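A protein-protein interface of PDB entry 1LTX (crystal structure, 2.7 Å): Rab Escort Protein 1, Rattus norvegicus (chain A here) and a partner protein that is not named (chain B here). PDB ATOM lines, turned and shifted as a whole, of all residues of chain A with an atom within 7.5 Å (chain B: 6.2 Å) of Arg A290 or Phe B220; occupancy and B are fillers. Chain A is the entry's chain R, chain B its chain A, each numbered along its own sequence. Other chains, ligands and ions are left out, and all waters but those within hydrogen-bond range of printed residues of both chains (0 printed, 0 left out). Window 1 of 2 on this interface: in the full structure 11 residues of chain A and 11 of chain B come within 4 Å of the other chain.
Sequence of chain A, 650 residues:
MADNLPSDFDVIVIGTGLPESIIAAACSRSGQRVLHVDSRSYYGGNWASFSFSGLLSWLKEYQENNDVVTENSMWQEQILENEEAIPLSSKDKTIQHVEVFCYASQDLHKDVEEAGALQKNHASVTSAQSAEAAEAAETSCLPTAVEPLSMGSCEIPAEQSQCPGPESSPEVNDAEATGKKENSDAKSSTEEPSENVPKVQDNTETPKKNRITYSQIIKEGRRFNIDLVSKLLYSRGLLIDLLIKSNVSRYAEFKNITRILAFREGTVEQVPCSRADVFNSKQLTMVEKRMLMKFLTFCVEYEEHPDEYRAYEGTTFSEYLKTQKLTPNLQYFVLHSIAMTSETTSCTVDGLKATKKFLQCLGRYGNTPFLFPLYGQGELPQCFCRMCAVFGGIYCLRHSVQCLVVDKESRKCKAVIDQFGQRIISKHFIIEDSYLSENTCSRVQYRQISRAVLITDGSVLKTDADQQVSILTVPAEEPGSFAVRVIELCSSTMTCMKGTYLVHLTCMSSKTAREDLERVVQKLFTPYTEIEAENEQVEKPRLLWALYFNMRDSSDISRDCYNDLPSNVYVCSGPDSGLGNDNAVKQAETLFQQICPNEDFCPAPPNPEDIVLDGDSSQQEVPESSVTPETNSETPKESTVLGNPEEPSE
NZ of Lys A289 is in hydrogen-bond range of OD1 of Asn B217, 3.4 Å away. O of Phe B220 is in hydrogen-bond range of NE of Arg A290. O of Thr B221 sits at hydrogen-bond distance from NH2 of Arg A290 (2.5 Å). The side-chain amino group (NZ) of Lys A294 sits at hydrogen-bond distance from the backbone carbonyl oxygen (O) of Leu B377, 3.3 Å away. OE1 of Glu B378 lies within salt-bridge range of NH1 of Arg A290 (3.3 Å). The side-chain carboxylate (OE2) of Glu B378 is in salt-bridge range of the side-chain amino group (NZ) of Lys A294, 2.6 Å away.
The backbone carbonyl oxygen (O) of Asn B217 lies within hydrogen-bond range of the side-chain hydroxyl (OG1) of Thr B221 (2.8 Å). The backbone carbonyl oxygen of Pro B223 lies within hydrogen-bond range of the indole nitrogen of Trp B229 (2.6 Å).
Among the printed residues, pairs that only touch across the chains: Val A287 with Glu B373, Met A286 with Phe B220, Met A293 with Thr B221, Met A286 with Asn B217, Arg A290 with Pro B223, Lys A325 with Leu B377, Arg A290 with Leu B377 and Met A291 with Leu B377.
Of the printed residues of chain B, Met A286 touches Asn B217 and Phe B220. Of the printed residues of chain B, Val A287 touches Glu B373. Of chain B, only Phe B220, Thr B221, Pro B223, Leu B377 and Glu B378 come within 4 Å of Arg A290. Leu A292 touches none of the printed residues of chain B. Printed residues of chain B within 4 Å of Lys A294: Leu B377 and Glu B378. Of the printed residues of chain A, Asn B217 touches Met A286 (3.4 Å) and Lys A289 (3.4 Å).
Of the 18 printed residues of chain B, 7 touch a printed residue of chain A. Hydrophobic or aromatic side chains of chain A that line the printed part of chain B: Met A286, Val A287, Met A291 and Met A293. Along chain A the printed residues that touch a printed residue of chain B span positions 286 to 325.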
ATOM      1  N   VAL A 278       3.318  18.646 -20.211  1.00  0.00           N
ATOM      2  CA  VAL A 278       3.230  19.698 -19.206  1.00  0.00           C
ATOM      3  C   VAL A 278       4.420  19.625 -18.264  1.00  0.00           C
ATOM      4  O   VAL A 278       5.052  20.643 -17.957  1.00  0.00           O
ATOM      5  CB  VAL A 278       1.963  19.563 -18.372  1.00  0.00           C
ATOM      6  CG1 VAL A 278       1.826  20.763 -17.457  1.00  0.00           C
ATOM      7  CG2 VAL A 278       0.764  19.426 -19.279  1.00  0.00           C
ATOM      8  N   LEU A 284       5.798  26.827 -19.358  1.00  0.00           N
ATOM      9  CA  LEU A 284       4.634  27.061 -18.522  1.00  0.00           C
ATOM     10  C   LEU A 284       5.072  27.309 -17.088  1.00  0.00           C
ATOM     11  O   LEU A 284       5.668  26.431 -16.459  1.00  0.00           O
ATOM     12  CB  LEU A 284       3.707  25.850 -18.544  1.00  0.00           C
ATOM     13  CG  LEU A 284       2.915  25.565 -19.815  1.00  0.00           C
ATOM     14  CD1 LEU A 284       3.855  25.488 -21.011  1.00  0.00           C
ATOM     15  CD2 LEU A 284       2.156  24.261 -19.632  1.00  0.00           C
ATOM     16  N   THR A 285       4.786  28.505 -16.576  1.00  0.00           N
ATOM     17  CA  THR A 285       5.121  28.842 -15.195  1.00  0.00           C
ATOM     18  C   THR A 285       4.565  27.716 -14.324  1.00  0.00           C
ATOM     19  O   THR A 285       3.506  27.154 -14.629  1.00  0.00           O
ATOM     20  CB  THR A 285       4.446  30.157 -14.744  1.00  0.00           C
ATOM     21  OG1 THR A 285       3.022  29.970 -14.677  1.00  0.00           O
ATOM     22  CG2 THR A 285       4.766  31.283 -15.711  1.00  0.00           C
ATOM     23  N   MET A 286       5.274  27.386 -13.247  1.00  0.00           N
ATOM     24  CA  MET A 286       4.841  26.321 -12.342  1.00  0.00           C
ATOM     25  C   MET A 286       3.328  26.386 -12.129  1.00  0.00           C
ATOM     26  O   MET A 286       2.631  25.371 -12.176  1.00  0.00           O
ATOM     27  CB  MET A 286       5.564  26.460 -11.004  1.00  0.00           C
ATOM     28  CG  MET A 286       5.958  25.136 -10.402  1.00  0.00           C
ATOM     29  SD  MET A 286       6.933  24.142 -11.561  1.00  0.00           S
ATOM     30  CE  MET A 286       8.414  25.163 -11.731  1.00  0.00           C
ATOM     31  N   VAL A 287       2.840  27.601 -11.917  1.00  0.00           N
ATOM     32  CA  VAL A 287       1.428  27.862 -11.698  1.00  0.00           C
ATOM     33  C   VAL A 287       0.578  27.368 -12.880  1.00  0.00           C
ATOM     34  O   VAL A 287      -0.454  26.705 -12.696  1.00  0.00           O
ATOM     35  CB  VAL A 287       1.198  29.379 -11.524  1.00  0.00           C
ATOM     36  CG1 VAL A 287      -0.099  29.631 -10.765  1.00  0.00           C
ATOM     37  CG2 VAL A 287       2.402  30.011 -10.817  1.00  0.00           C
ATOM     38  N   GLU A 288       1.012  27.695 -14.095  1.00  0.00           N
ATOM     39  CA  GLU A 288       0.278  27.293 -15.289  1.00  0.00           C
ATOM     40  C   GLU A 288       0.125  25.790 -15.389  1.00  0.00           C
ATOM     41  O   GLU A 288      -0.971  25.291 -15.630  1.00  0.00           O
ATOM     42  CB  GLU A 288       0.971  27.821 -16.543  1.00  0.00           C
ATOM     43  CG  GLU A 288       0.985  29.339 -16.641  1.00  0.00           C
ATOM     44  CD  GLU A 288       1.617  29.836 -17.929  1.00  0.00           C
ATOM     45  OE1 GLU A 288       2.738  29.388 -18.260  1.00  0.00           O
ATOM     46  OE2 GLU A 288       0.994  30.681 -18.606  1.00  0.00           O
ATOM     47  N   LYS A 289       1.222  25.070 -15.196  1.00  0.00           N
ATOM     48  CA  LYS A 289       1.182  23.619 -15.274  1.00  0.00           C
ATOM     49  C   LYS A 289       0.033  23.055 -14.451  1.00  0.00           C
ATOM     50  O   LYS A 289      -0.531  22.008 -14.775  1.00  0.00           O
ATOM     51  CB  LYS A 289       2.494  23.032 -14.784  1.00  0.00           C
ATOM     52  CG  LYS A 289       3.708  23.633 -15.446  1.00  0.00           C
ATOM     53  CD  LYS A 289       4.923  22.762 -15.182  1.00  0.00           C
ATOM     54  CE  LYS A 289       6.175  23.329 -15.820  1.00  0.00           C
ATOM     55  NZ  LYS A 289       7.280  22.340 -15.750  1.00  0.00           N
ATOM     56  N   ARG A 290      -0.321  23.753 -13.383  1.00  0.00           N
ATOM     57  CA  ARG A 290      -1.407  23.295 -12.538  1.00  0.00           C
ATOM     58  C   ARG A 290      -2.747  23.615 -13.184  1.00  0.00           C
ATOM     59  O   ARG A 290      -3.602  22.731 -13.333  1.00  0.00           O
ATOM     60  CB  ARG A 290      -1.333  23.966 -11.167  1.00  0.00           C
ATOM     61  CG  ARG A 290      -1.374  23.004  -9.984  1.00  0.00           C
ATOM     62  CD  ARG A 290      -2.628  22.142  -9.960  1.00  0.00           C
ATOM     63  NE  ARG A 290      -2.461  20.883 -10.677  1.00  0.00           N
ATOM     64  CZ  ARG A 290      -3.445  20.001 -10.853  1.00  0.00           C
ATOM     65  NH1 ARG A 290      -4.658  20.254 -10.359  1.00  0.00           N
ATOM     66  NH2 ARG A 290      -3.231  18.873 -11.524  1.00  0.00           N
ATOM     67  N   MET A 291      -2.923  24.884 -13.554  1.00  0.00           N
ATOM     68  CA  MET A 291      -4.163  25.347 -14.177  1.00  0.00           C
ATOM     69  C   MET A 291      -4.553  24.458 -15.341  1.00  0.00           C
ATOM     70  O   MET A 291      -5.667  23.929 -15.404  1.00  0.00           O
ATOM     71  CB  MET A 291      -3.996  26.783 -14.672  1.00  0.00           C
ATOM     72  CG  MET A 291      -3.769  27.768 -13.558  1.00  0.00           C
ATOM     73  SD  MET A 291      -3.516  29.447 -14.145  1.00  0.00           S
ATOM     74  CE  MET A 291      -1.806  29.737 -13.677  1.00  0.00           C
ATOM     75  N   LEU A 292      -3.611  24.293 -16.259  1.00  0.00           N
ATOM     76  CA  LEU A 292      -3.840  23.484 -17.436  1.00  0.00           C
ATOM     77  C   LEU A 292      -4.218  22.062 -17.072  1.00  0.00           C
ATOM     78  O   LEU A 292      -5.283  21.573 -17.453  1.00  0.00           O
ATOM     79  CB  LEU A 292      -2.593  23.476 -18.322  1.00  0.00           C
ATOM     80  CG  LEU A 292      -2.711  22.606 -19.577  1.00  0.00           C
ATOM     81  CD1 LEU A 292      -3.892  23.087 -20.401  1.00  0.00           C
ATOM     82  CD2 LEU A 292      -1.416  22.657 -20.371  1.00  0.00           C
ATOM     83  N   MET A 293      -3.332  21.406 -16.334  1.00  0.00           N
ATOM     84  CA  MET A 293      -3.533  20.030 -15.908  1.00  0.00           C
ATOM     85  C   MET A 293      -4.870  19.875 -15.198  1.00  0.00           C
ATOM     86  O   MET A 293      -5.578  18.882 -15.374  1.00  0.00           O
ATOM     87  CB  MET A 293      -2.402  19.635 -14.981  1.00  0.00           C
ATOM     88  CG  MET A 293      -1.965  18.219 -15.157  1.00  0.00           C
ATOM     89  SD  MET A 293      -1.455  17.920 -16.855  1.00  0.00           S
ATOM     90  CE  MET A 293      -2.765  16.792 -17.354  1.00  0.00           C
ATOM     91  N   LYS A 294      -5.210  20.879 -14.401  1.00  0.00           N
ATOM     92  CA  LYS A 294      -6.462  20.885 -13.659  1.00  0.00           C
ATOM     93  C   LYS A 294      -7.644  20.957 -14.611  1.00  0.00           C
ATOM     94  O   LYS A 294      -8.521  20.094 -14.588  1.00  0.00           O
ATOM     95  CB  LYS A 294      -6.499  22.092 -12.712  1.00  0.00           C
ATOM     96  CG  LYS A 294      -7.788  22.249 -11.909  1.00  0.00           C
ATOM     97  CD  LYS A 294      -7.804  23.612 -11.189  1.00  0.00           C
ATOM     98  CE  LYS A 294      -8.845  23.685 -10.060  1.00  0.00           C
ATOM     99  NZ  LYS A 294      -8.494  22.826  -8.883  1.00  0.00           N
ATOM    100  N   PHE A 295      -7.644  21.989 -15.453  1.00  0.00           N
ATOM    101  CA  PHE A 295      -8.720  22.233 -16.411  1.00  0.00           C
ATOM    102  C   PHE A 295      -8.940  21.113 -17.411  1.00  0.00           C
ATOM    103  O   PHE A 295     -10.084  20.741 -17.681  1.00  0.00           O
ATOM    104  CB  PHE A 295      -8.463  23.546 -17.154  1.00  0.00           C
ATOM    105  CG  PHE A 295      -9.549  23.923 -18.122  1.00  0.00           C
ATOM    106  CD1 PHE A 295      -9.492  23.510 -19.455  1.00  0.00           C
ATOM    107  CD2 PHE A 295     -10.639  24.682 -17.704  1.00  0.00           C
ATOM    108  CE1 PHE A 295     -10.503  23.851 -20.355  1.00  0.00           C
ATOM    109  CE2 PHE A 295     -11.658  25.027 -18.600  1.00  0.00           C
ATOM    110  CZ  PHE A 295     -11.586  24.608 -19.928  1.00  0.00           C
ATOM    111  N   LEU A 296      -7.854  20.582 -17.967  1.00  0.00           N
ATOM    112  CA  LEU A 296      -7.975  19.498 -18.933  1.00  0.00           C
ATOM    113  C   LEU A 296      -8.623  18.299 -18.273  1.00  0.00           C
ATOM    114  O   LEU A 296      -9.492  17.656 -18.865  1.00  0.00           O
ATOM    115  CB  LEU A 296      -6.613  19.102 -19.509  1.00  0.00           C
ATOM    116  CG  LEU A 296      -5.956  20.105 -20.462  1.00  0.00           C
ATOM    117  CD1 LEU A 296      -4.694  19.489 -21.028  1.00  0.00           C
ATOM    118  CD2 LEU A 296      -6.913  20.480 -21.595  1.00  0.00           C
ATOM    119  N   THR A 297      -8.212  18.005 -17.040  1.00  0.00           N
ATOM    120  CA  THR A 297      -8.787  16.878 -16.318  1.00  0.00           C
ATOM    121  C   THR A 297     -10.286  17.129 -16.165  1.00  0.00           C
ATOM    122  O   THR A 297     -11.073  16.199 -15.993  1.00  0.00           O
ATOM    123  CB  THR A 297      -8.144  16.703 -14.932  1.00  0.00           C
ATOM    124  OG1 THR A 297      -6.720  16.818 -15.045  1.00  0.00           O
ATOM    125  CG2 THR A 297      -8.474  15.324 -14.379  1.00  0.00           C
ATOM    126  N   LYS A 325      -9.854  29.380 -14.685  1.00  0.00           N
ATOM    127  CA  LYS A 325      -8.536  29.554 -14.098  1.00  0.00           C
ATOM    128  C   LYS A 325      -7.442  29.148 -15.083  1.00  0.00           C
ATOM    129  O   LYS A 325      -6.756  28.133 -14.907  1.00  0.00           O
ATOM    130  CB  LYS A 325      -8.430  28.736 -12.810  1.00  0.00           C
ATOM    131  CG  LYS A 325      -9.037  29.423 -11.586  1.00  0.00           C
ATOM    132  CD  LYS A 325      -9.065  28.501 -10.382  1.00  0.00           C
ATOM    133  CE  LYS A 325     -10.240  27.541 -10.456  1.00  0.00           C
ATOM    134  NZ  LYS A 325     -11.525  28.274 -10.266  1.00  0.00           N
ATOM    135  N   LEU A 326      -7.298  29.953 -16.128  1.00  0.00           N
ATOM    136  CA  LEU A 326      -6.308  29.722 -17.171  1.00  0.00           C
ATOM    137  C   LEU A 326      -5.677  31.048 -17.532  1.00  0.00           C
ATOM    138  O   LEU A 326      -6.373  32.050 -17.664  1.00  0.00           O
ATOM    139  CB  LEU A 326      -6.960  29.155 -18.448  1.00  0.00           C
ATOM    140  CG  LEU A 326      -7.581  27.759 -18.555  1.00  0.00           C
ATOM    141  CD1 LEU A 326      -6.542  26.709 -18.219  1.00  0.00           C
ATOM    142  CD2 LEU A 326      -8.767  27.641 -17.637  1.00  0.00           C
ATOM    143  N   LEU A 330      -2.543  29.863 -21.817  1.00  0.00           N
ATOM    144  CA  LEU A 330      -3.209  28.569 -21.800  1.00  0.00           C
ATOM    145  C   LEU A 330      -4.570  28.635 -22.461  1.00  0.00           C
ATOM    146  O   LEU A 330      -5.074  27.624 -22.951  1.00  0.00           O
ATOM    147  CB  LEU A 330      -3.367  28.064 -20.366  1.00  0.00           C
ATOM    148  CG  LEU A 330      -2.102  27.844 -19.538  1.00  0.00           C
ATOM    149  CD1 LEU A 330      -2.522  27.224 -18.215  1.00  0.00           C
ATOM    150  CD2 LEU A 330      -1.123  26.936 -20.257  1.00  0.00           C
ATOM    151  N   VAL B 215      11.146  18.000  -8.588  1.00  0.00           N
ATOM    152  CA  VAL B 215      10.012  17.603  -7.750  1.00  0.00           C
ATOM    153  C   VAL B 215       8.954  18.710  -7.662  1.00  0.00           C
ATOM    154  O   VAL B 215       7.751  18.429  -7.644  1.00  0.00           O
ATOM    155  CB  VAL B 215      10.479  17.186  -6.307  1.00  0.00           C
ATOM    156  CG1 VAL B 215      10.661  18.408  -5.413  1.00  0.00           C
ATOM    157  CG2 VAL B 215       9.477  16.216  -5.706  1.00  0.00           C
ATOM    158  N   GLN B 216       9.410  19.960  -7.633  1.00  0.00           N
ATOM    159  CA  GLN B 216       8.507  21.098  -7.544  1.00  0.00           C
ATOM    160  C   GLN B 216       7.398  21.029  -8.580  1.00  0.00           C
ATOM    161  O   GLN B 216       6.283  21.477  -8.324  1.00  0.00           O
ATOM    162  CB  GLN B 216       9.273  22.409  -7.711  1.00  0.00           C
ATOM    163  CG  GLN B 216       8.409  23.653  -7.535  1.00  0.00           C
ATOM    164  CD  GLN B 216       9.215  24.942  -7.607  1.00  0.00           C
ATOM    165  OE1 GLN B 216       8.670  26.037  -7.461  1.00  0.00           O
ATOM    166  NE2 GLN B 216      10.522  24.815  -7.834  1.00  0.00           N
ATOM    167  N   ASN B 217       7.685  20.473  -9.751  1.00  0.00           N
ATOM    168  CA  ASN B 217       6.642  20.388 -10.760  1.00  0.00           C
ATOM    169  C   ASN B 217       6.002  19.012 -10.782  1.00  0.00           C
ATOM    170  O   ASN B 217       4.948  18.817 -11.377  1.00  0.00           O
ATOM    171  CB  ASN B 217       7.183  20.761 -12.153  1.00  0.00           C
ATOM    172  CG  ASN B 217       8.223  19.787 -12.674  1.00  0.00           C
ATOM    173  OD1 ASN B 217       8.760  19.971 -13.769  1.00  0.00           O
ATOM    174  ND2 ASN B 217       8.513  18.748 -11.898  1.00  0.00           N
ATOM    175  N   ALA B 218       6.631  18.054 -10.121  1.00  0.00           N
ATOM    176  CA  ALA B 218       6.071  16.712 -10.083  1.00  0.00           C
ATOM    177  C   ALA B 218       4.710  16.769  -9.403  1.00  0.00           C
ATOM    178  O   ALA B 218       3.773  16.064  -9.796  1.00  0.00           O
ATOM    179  CB  ALA B 218       6.996  15.776  -9.326  1.00  0.00           C
ATOM    180  N   PHE B 219       4.604  17.619  -8.381  1.00  0.00           N
ATOM    181  CA  PHE B 219       3.354  17.756  -7.645  1.00  0.00           C
ATOM    182  C   PHE B 219       2.512  18.950  -8.095  1.00  0.00           C
ATOM    183  O   PHE B 219       1.319  19.033  -7.773  1.00  0.00           O
ATOM    184  CB  PHE B 219       3.607  17.794  -6.117  1.00  0.00           C
ATOM    185  CG  PHE B 219       4.562  18.883  -5.649  1.00  0.00           C
ATOM    186  CD1 PHE B 219       4.287  20.229  -5.869  1.00  0.00           C
ATOM    187  CD2 PHE B 219       5.712  18.548  -4.926  1.00  0.00           C
ATOM    188  CE1 PHE B 219       5.142  21.225  -5.374  1.00  0.00           C
ATOM    189  CE2 PHE B 219       6.569  19.537  -4.430  1.00  0.00           C
ATOM    190  CZ  PHE B 219       6.283  20.874  -4.654  1.00  0.00           C
ATOM    191  N   PHE B 220       3.124  19.874  -8.836  1.00  0.00           N
ATOM    192  CA  PHE B 220       2.381  21.018  -9.356  1.00  0.00           C
ATOM    193  C   PHE B 220       1.558  20.478 -10.525  1.00  0.00           C
ATOM    194  O   PHE B 220       0.415  20.880 -10.743  1.00  0.00           O
ATOM    195  CB  PHE B 220       3.331  22.103  -9.826  1.00  0.00           C
ATOM    196  CG  PHE B 220       3.301  23.340  -8.979  1.00  0.00           C
ATOM    197  CD1 PHE B 220       2.257  24.245  -9.093  1.00  0.00           C
ATOM    198  CD2 PHE B 220       4.340  23.622  -8.097  1.00  0.00           C
ATOM    199  CE1 PHE B 220       2.247  25.420  -8.355  1.00  0.00           C
ATOM    200  CE2 PHE B 220       4.341  24.794  -7.352  1.00  0.00           C
ATOM    201  CZ  PHE B 220       3.288  25.696  -7.486  1.00  0.00           C
ATOM    202  N   THR B 221       2.154  19.546 -11.264  1.00  0.00           N
ATOM    203  CA  THR B 221       1.469  18.901 -12.372  1.00  0.00           C
ATOM    204  C   THR B 221       0.356  18.111 -11.712  1.00  0.00           C
ATOM    205  O   THR B 221      -0.815  18.314 -12.010  1.00  0.00           O
ATOM    206  CB  THR B 221       2.394  17.916 -13.129  1.00  0.00           C
ATOM    207  OG1 THR B 221       3.445  18.646 -13.772  1.00  0.00           O
ATOM    208  CG2 THR B 221       1.607  17.125 -14.179  1.00  0.00           C
ATOM    209  N   ASP B 222       0.741  17.221 -10.797  1.00  0.00           N
ATOM    210  CA  ASP B 222      -0.203  16.373 -10.057  1.00  0.00           C
ATOM    211  C   ASP B 222       0.059  16.440  -8.532  1.00  0.00           C
ATOM    212  O   ASP B 222       0.939  15.744  -8.012  1.00  0.00           O
ATOM    213  CB  ASP B 222      -0.088  14.925 -10.561  1.00  0.00           C
ATOM    214  CG  ASP B 222      -1.064  13.980  -9.874  1.00  0.00           C
ATOM    215  OD1 ASP B 222      -2.189  14.423  -9.540  1.00  0.00           O
ATOM    216  OD2 ASP B 222      -0.713  12.789  -9.686  1.00  0.00           O
ATOM    217  N   PRO B 223      -0.699  17.286  -7.802  1.00  0.00           N
ATOM    218  CA  PRO B 223      -0.540  17.439  -6.354  1.00  0.00           C
ATOM    219  C   PRO B 223      -1.175  16.333  -5.528  1.00  0.00           C
ATOM    220  O   PRO B 223      -0.958  16.270  -4.322  1.00  0.00           O
ATOM    221  CB  PRO B 223      -1.187  18.790  -6.085  1.00  0.00           C
ATOM    222  CG  PRO B 223      -2.342  18.763  -7.021  1.00  0.00           C
ATOM    223  CD  PRO B 223      -1.703  18.240  -8.306  1.00  0.00           C
ATOM    224  N   ASN B 224      -1.964  15.472  -6.164  1.00  0.00           N
ATOM    225  CA  ASN B 224      -2.602  14.374  -5.449  1.00  0.00           C
ATOM    226  C   ASN B 224      -1.752  13.128  -5.518  1.00  0.00           C
ATOM    227  O   ASN B 224      -2.246  12.005  -5.397  1.00  0.00           O
ATOM    228  CB  ASN B 224      -3.982  14.069  -6.016  1.00  0.00           C
ATOM    229  CG  ASN B 224      -4.938  15.230  -5.871  1.00  0.00           C
ATOM    230  OD1 ASN B 224      -6.154  15.039  -5.907  1.00  0.00           O
ATOM    231  ND2 ASN B 224      -4.398  16.444  -5.718  1.00  0.00           N
ATOM    232  N   TRP B 229       5.375  14.632  -2.835  1.00  0.00           N
ATOM    233  CA  TRP B 229       5.303  15.265  -1.520  1.00  0.00           C
ATOM    234  C   TRP B 229       6.256  14.680  -0.486  1.00  0.00           C
ATOM    235  O   TRP B 229       6.972  15.427   0.184  1.00  0.00           O
ATOM    236  CB  TRP B 229       3.869  15.197  -1.020  1.00  0.00           C
ATOM    237  CG  TRP B 229       2.943  16.069  -1.808  1.00  0.00           C
ATOM    238  CD1 TRP B 229       1.777  15.693  -2.416  1.00  0.00           C
ATOM    239  CD2 TRP B 229       3.076  17.481  -2.029  1.00  0.00           C
ATOM    240  NE1 TRP B 229       1.173  16.787  -2.994  1.00  0.00           N
ATOM    241  CE2 TRP B 229       1.947  17.896  -2.769  1.00  0.00           C
ATOM    242  CE3 TRP B 229       4.039  18.436  -1.670  1.00  0.00           C
ATOM    243  CZ2 TRP B 229       1.748  19.227  -3.157  1.00  0.00           C
ATOM    244  CZ3 TRP B 229       3.843  19.769  -2.057  1.00  0.00           C
ATOM    245  CH2 TRP B 229       2.701  20.148  -2.794  1.00  0.00           C
ATOM    246  N   GLU B 367      10.285  28.686  -3.624  1.00  0.00           N
ATOM    247  CA  GLU B 367       9.554  27.437  -3.444  1.00  0.00           C
ATOM    248  C   GLU B 367       8.301  27.724  -2.622  1.00  0.00           C
ATOM    249  O   GLU B 367       7.191  27.302  -2.967  1.00  0.00           O
ATOM    250  CB  GLU B 367      10.455  26.431  -2.711  1.00  0.00           C
ATOM    251  CG  GLU B 367       9.847  25.056  -2.499  1.00  0.00           C
ATOM    252  CD  GLU B 367       9.801  24.227  -3.765  1.00  0.00           C
ATOM    253  OE1 GLU B 367      10.804  23.530  -4.064  1.00  0.00           O
ATOM    254  OE2 GLU B 367       8.760  24.280  -4.459  1.00  0.00           O
ATOM    255  N   SER B 370       5.544  29.980  -4.455  1.00  0.00           N
ATOM    256  CA  SER B 370       4.852  29.171  -5.450  1.00  0.00           C
ATOM    257  C   SER B 370       3.810  28.251  -4.812  1.00  0.00           C
ATOM    258  O   SER B 370       2.768  27.962  -5.414  1.00  0.00           O
ATOM    259  CB  SER B 370       5.855  28.329  -6.242  1.00  0.00           C
ATOM    260  OG  SER B 370       6.863  29.144  -6.812  1.00  0.00           O
ATOM    261  N   CYS B 371       4.082  27.804  -3.587  1.00  0.00           N
ATOM    262  CA  CYS B 371       3.171  26.893  -2.899  1.00  0.00           C
ATOM    263  C   CYS B 371       1.902  27.530  -2.356  1.00  0.00           C
ATOM    264  O   CYS B 371       0.861  26.874  -2.274  1.00  0.00           O
ATOM    265  CB  CYS B 371       3.914  26.156  -1.792  1.00  0.00           C
ATOM    266  SG  CYS B 371       5.063  24.950  -2.460  1.00  0.00           S
ATOM    267  N   GLU B 373       0.386  29.747  -3.876  1.00  0.00           N
ATOM    268  CA  GLU B 373      -0.425  29.817  -5.090  1.00  0.00           C
ATOM    269  C   GLU B 373      -1.139  28.493  -5.284  1.00  0.00           C
ATOM    270  O   GLU B 373      -2.346  28.452  -5.519  1.00  0.00           O
ATOM    271  CB  GLU B 373       0.451  30.078  -6.314  1.00  0.00           C
ATOM    272  CG  GLU B 373       1.220  31.381  -6.288  1.00  0.00           C
ATOM    273  CD  GLU B 373       2.010  31.596  -7.563  1.00  0.00           C
ATOM    274  OE1 GLU B 373       1.377  31.662  -8.642  1.00  0.00           O
ATOM    275  OE2 GLU B 373       3.259  31.691  -7.490  1.00  0.00           O
ATOM    276  N   LEU B 374      -0.369  27.412  -5.185  1.00  0.00           N
ATOM    277  CA  LEU B 374      -0.892  26.062  -5.354  1.00  0.00           C
ATOM    278  C   LEU B 374      -2.050  25.832  -4.394  1.00  0.00           C
ATOM    279  O   LEU B 374      -2.961  25.039  -4.651  1.00  0.00           O
ATOM    280  CB  LEU B 374       0.214  25.048  -5.076  1.00  0.00           C
ATOM    281  CG  LEU B 374       0.252  23.773  -5.917  1.00  0.00           C
ATOM    282  CD1 LEU B 374       1.302  22.852  -5.323  1.00  0.00           C
ATOM    283  CD2 LEU B 374      -1.105  23.085  -5.945  1.00  0.00           C
ATOM    284  N   LEU B 377      -5.310  27.441  -5.735  1.00  0.00           N
ATOM    285  CA  LEU B 377      -5.858  26.556  -6.758  1.00  0.00           C
ATOM    286  C   LEU B 377      -6.381  25.278  -6.122  1.00  0.00           C
ATOM    287  O   LEU B 377      -7.500  24.843  -6.404  1.00  0.00           O
ATOM    288  CB  LEU B 377      -4.783  26.206  -7.791  1.00  0.00           C
ATOM    289  CG  LEU B 377      -4.583  27.179  -8.956  1.00  0.00           C
ATOM    290  CD1 LEU B 377      -3.318  26.811  -9.732  1.00  0.00           C
ATOM    291  CD2 LEU B 377      -5.817  27.136  -9.865  1.00  0.00           C
ATOM    292  N   GLU B 378      -5.547  24.674  -5.276  1.00  0.00           N
ATOM    293  CA  GLU B 378      -5.901  23.450  -4.554  1.00  0.00           C
ATOM    294  C   GLU B 378      -5.961  23.801  -3.067  1.00  0.00           C
ATOM    295  O   GLU B 378      -5.000  23.595  -2.326  1.00  0.00           O
ATOM    296  CB  GLU B 378      -4.849  22.361  -4.790  1.00  0.00           C
ATOM    297  CG  GLU B 378      -5.292  21.225  -5.712  1.00  0.00           C
ATOM    298  CD  GLU B 378      -5.615  21.692  -7.126  1.00  0.00           C
ATOM    299  OE1 GLU B 378      -4.734  22.300  -7.777  1.00  0.00           O
ATOM    300  OE2 GLU B 378      -6.753  21.448  -7.588  1.00  0.00           O
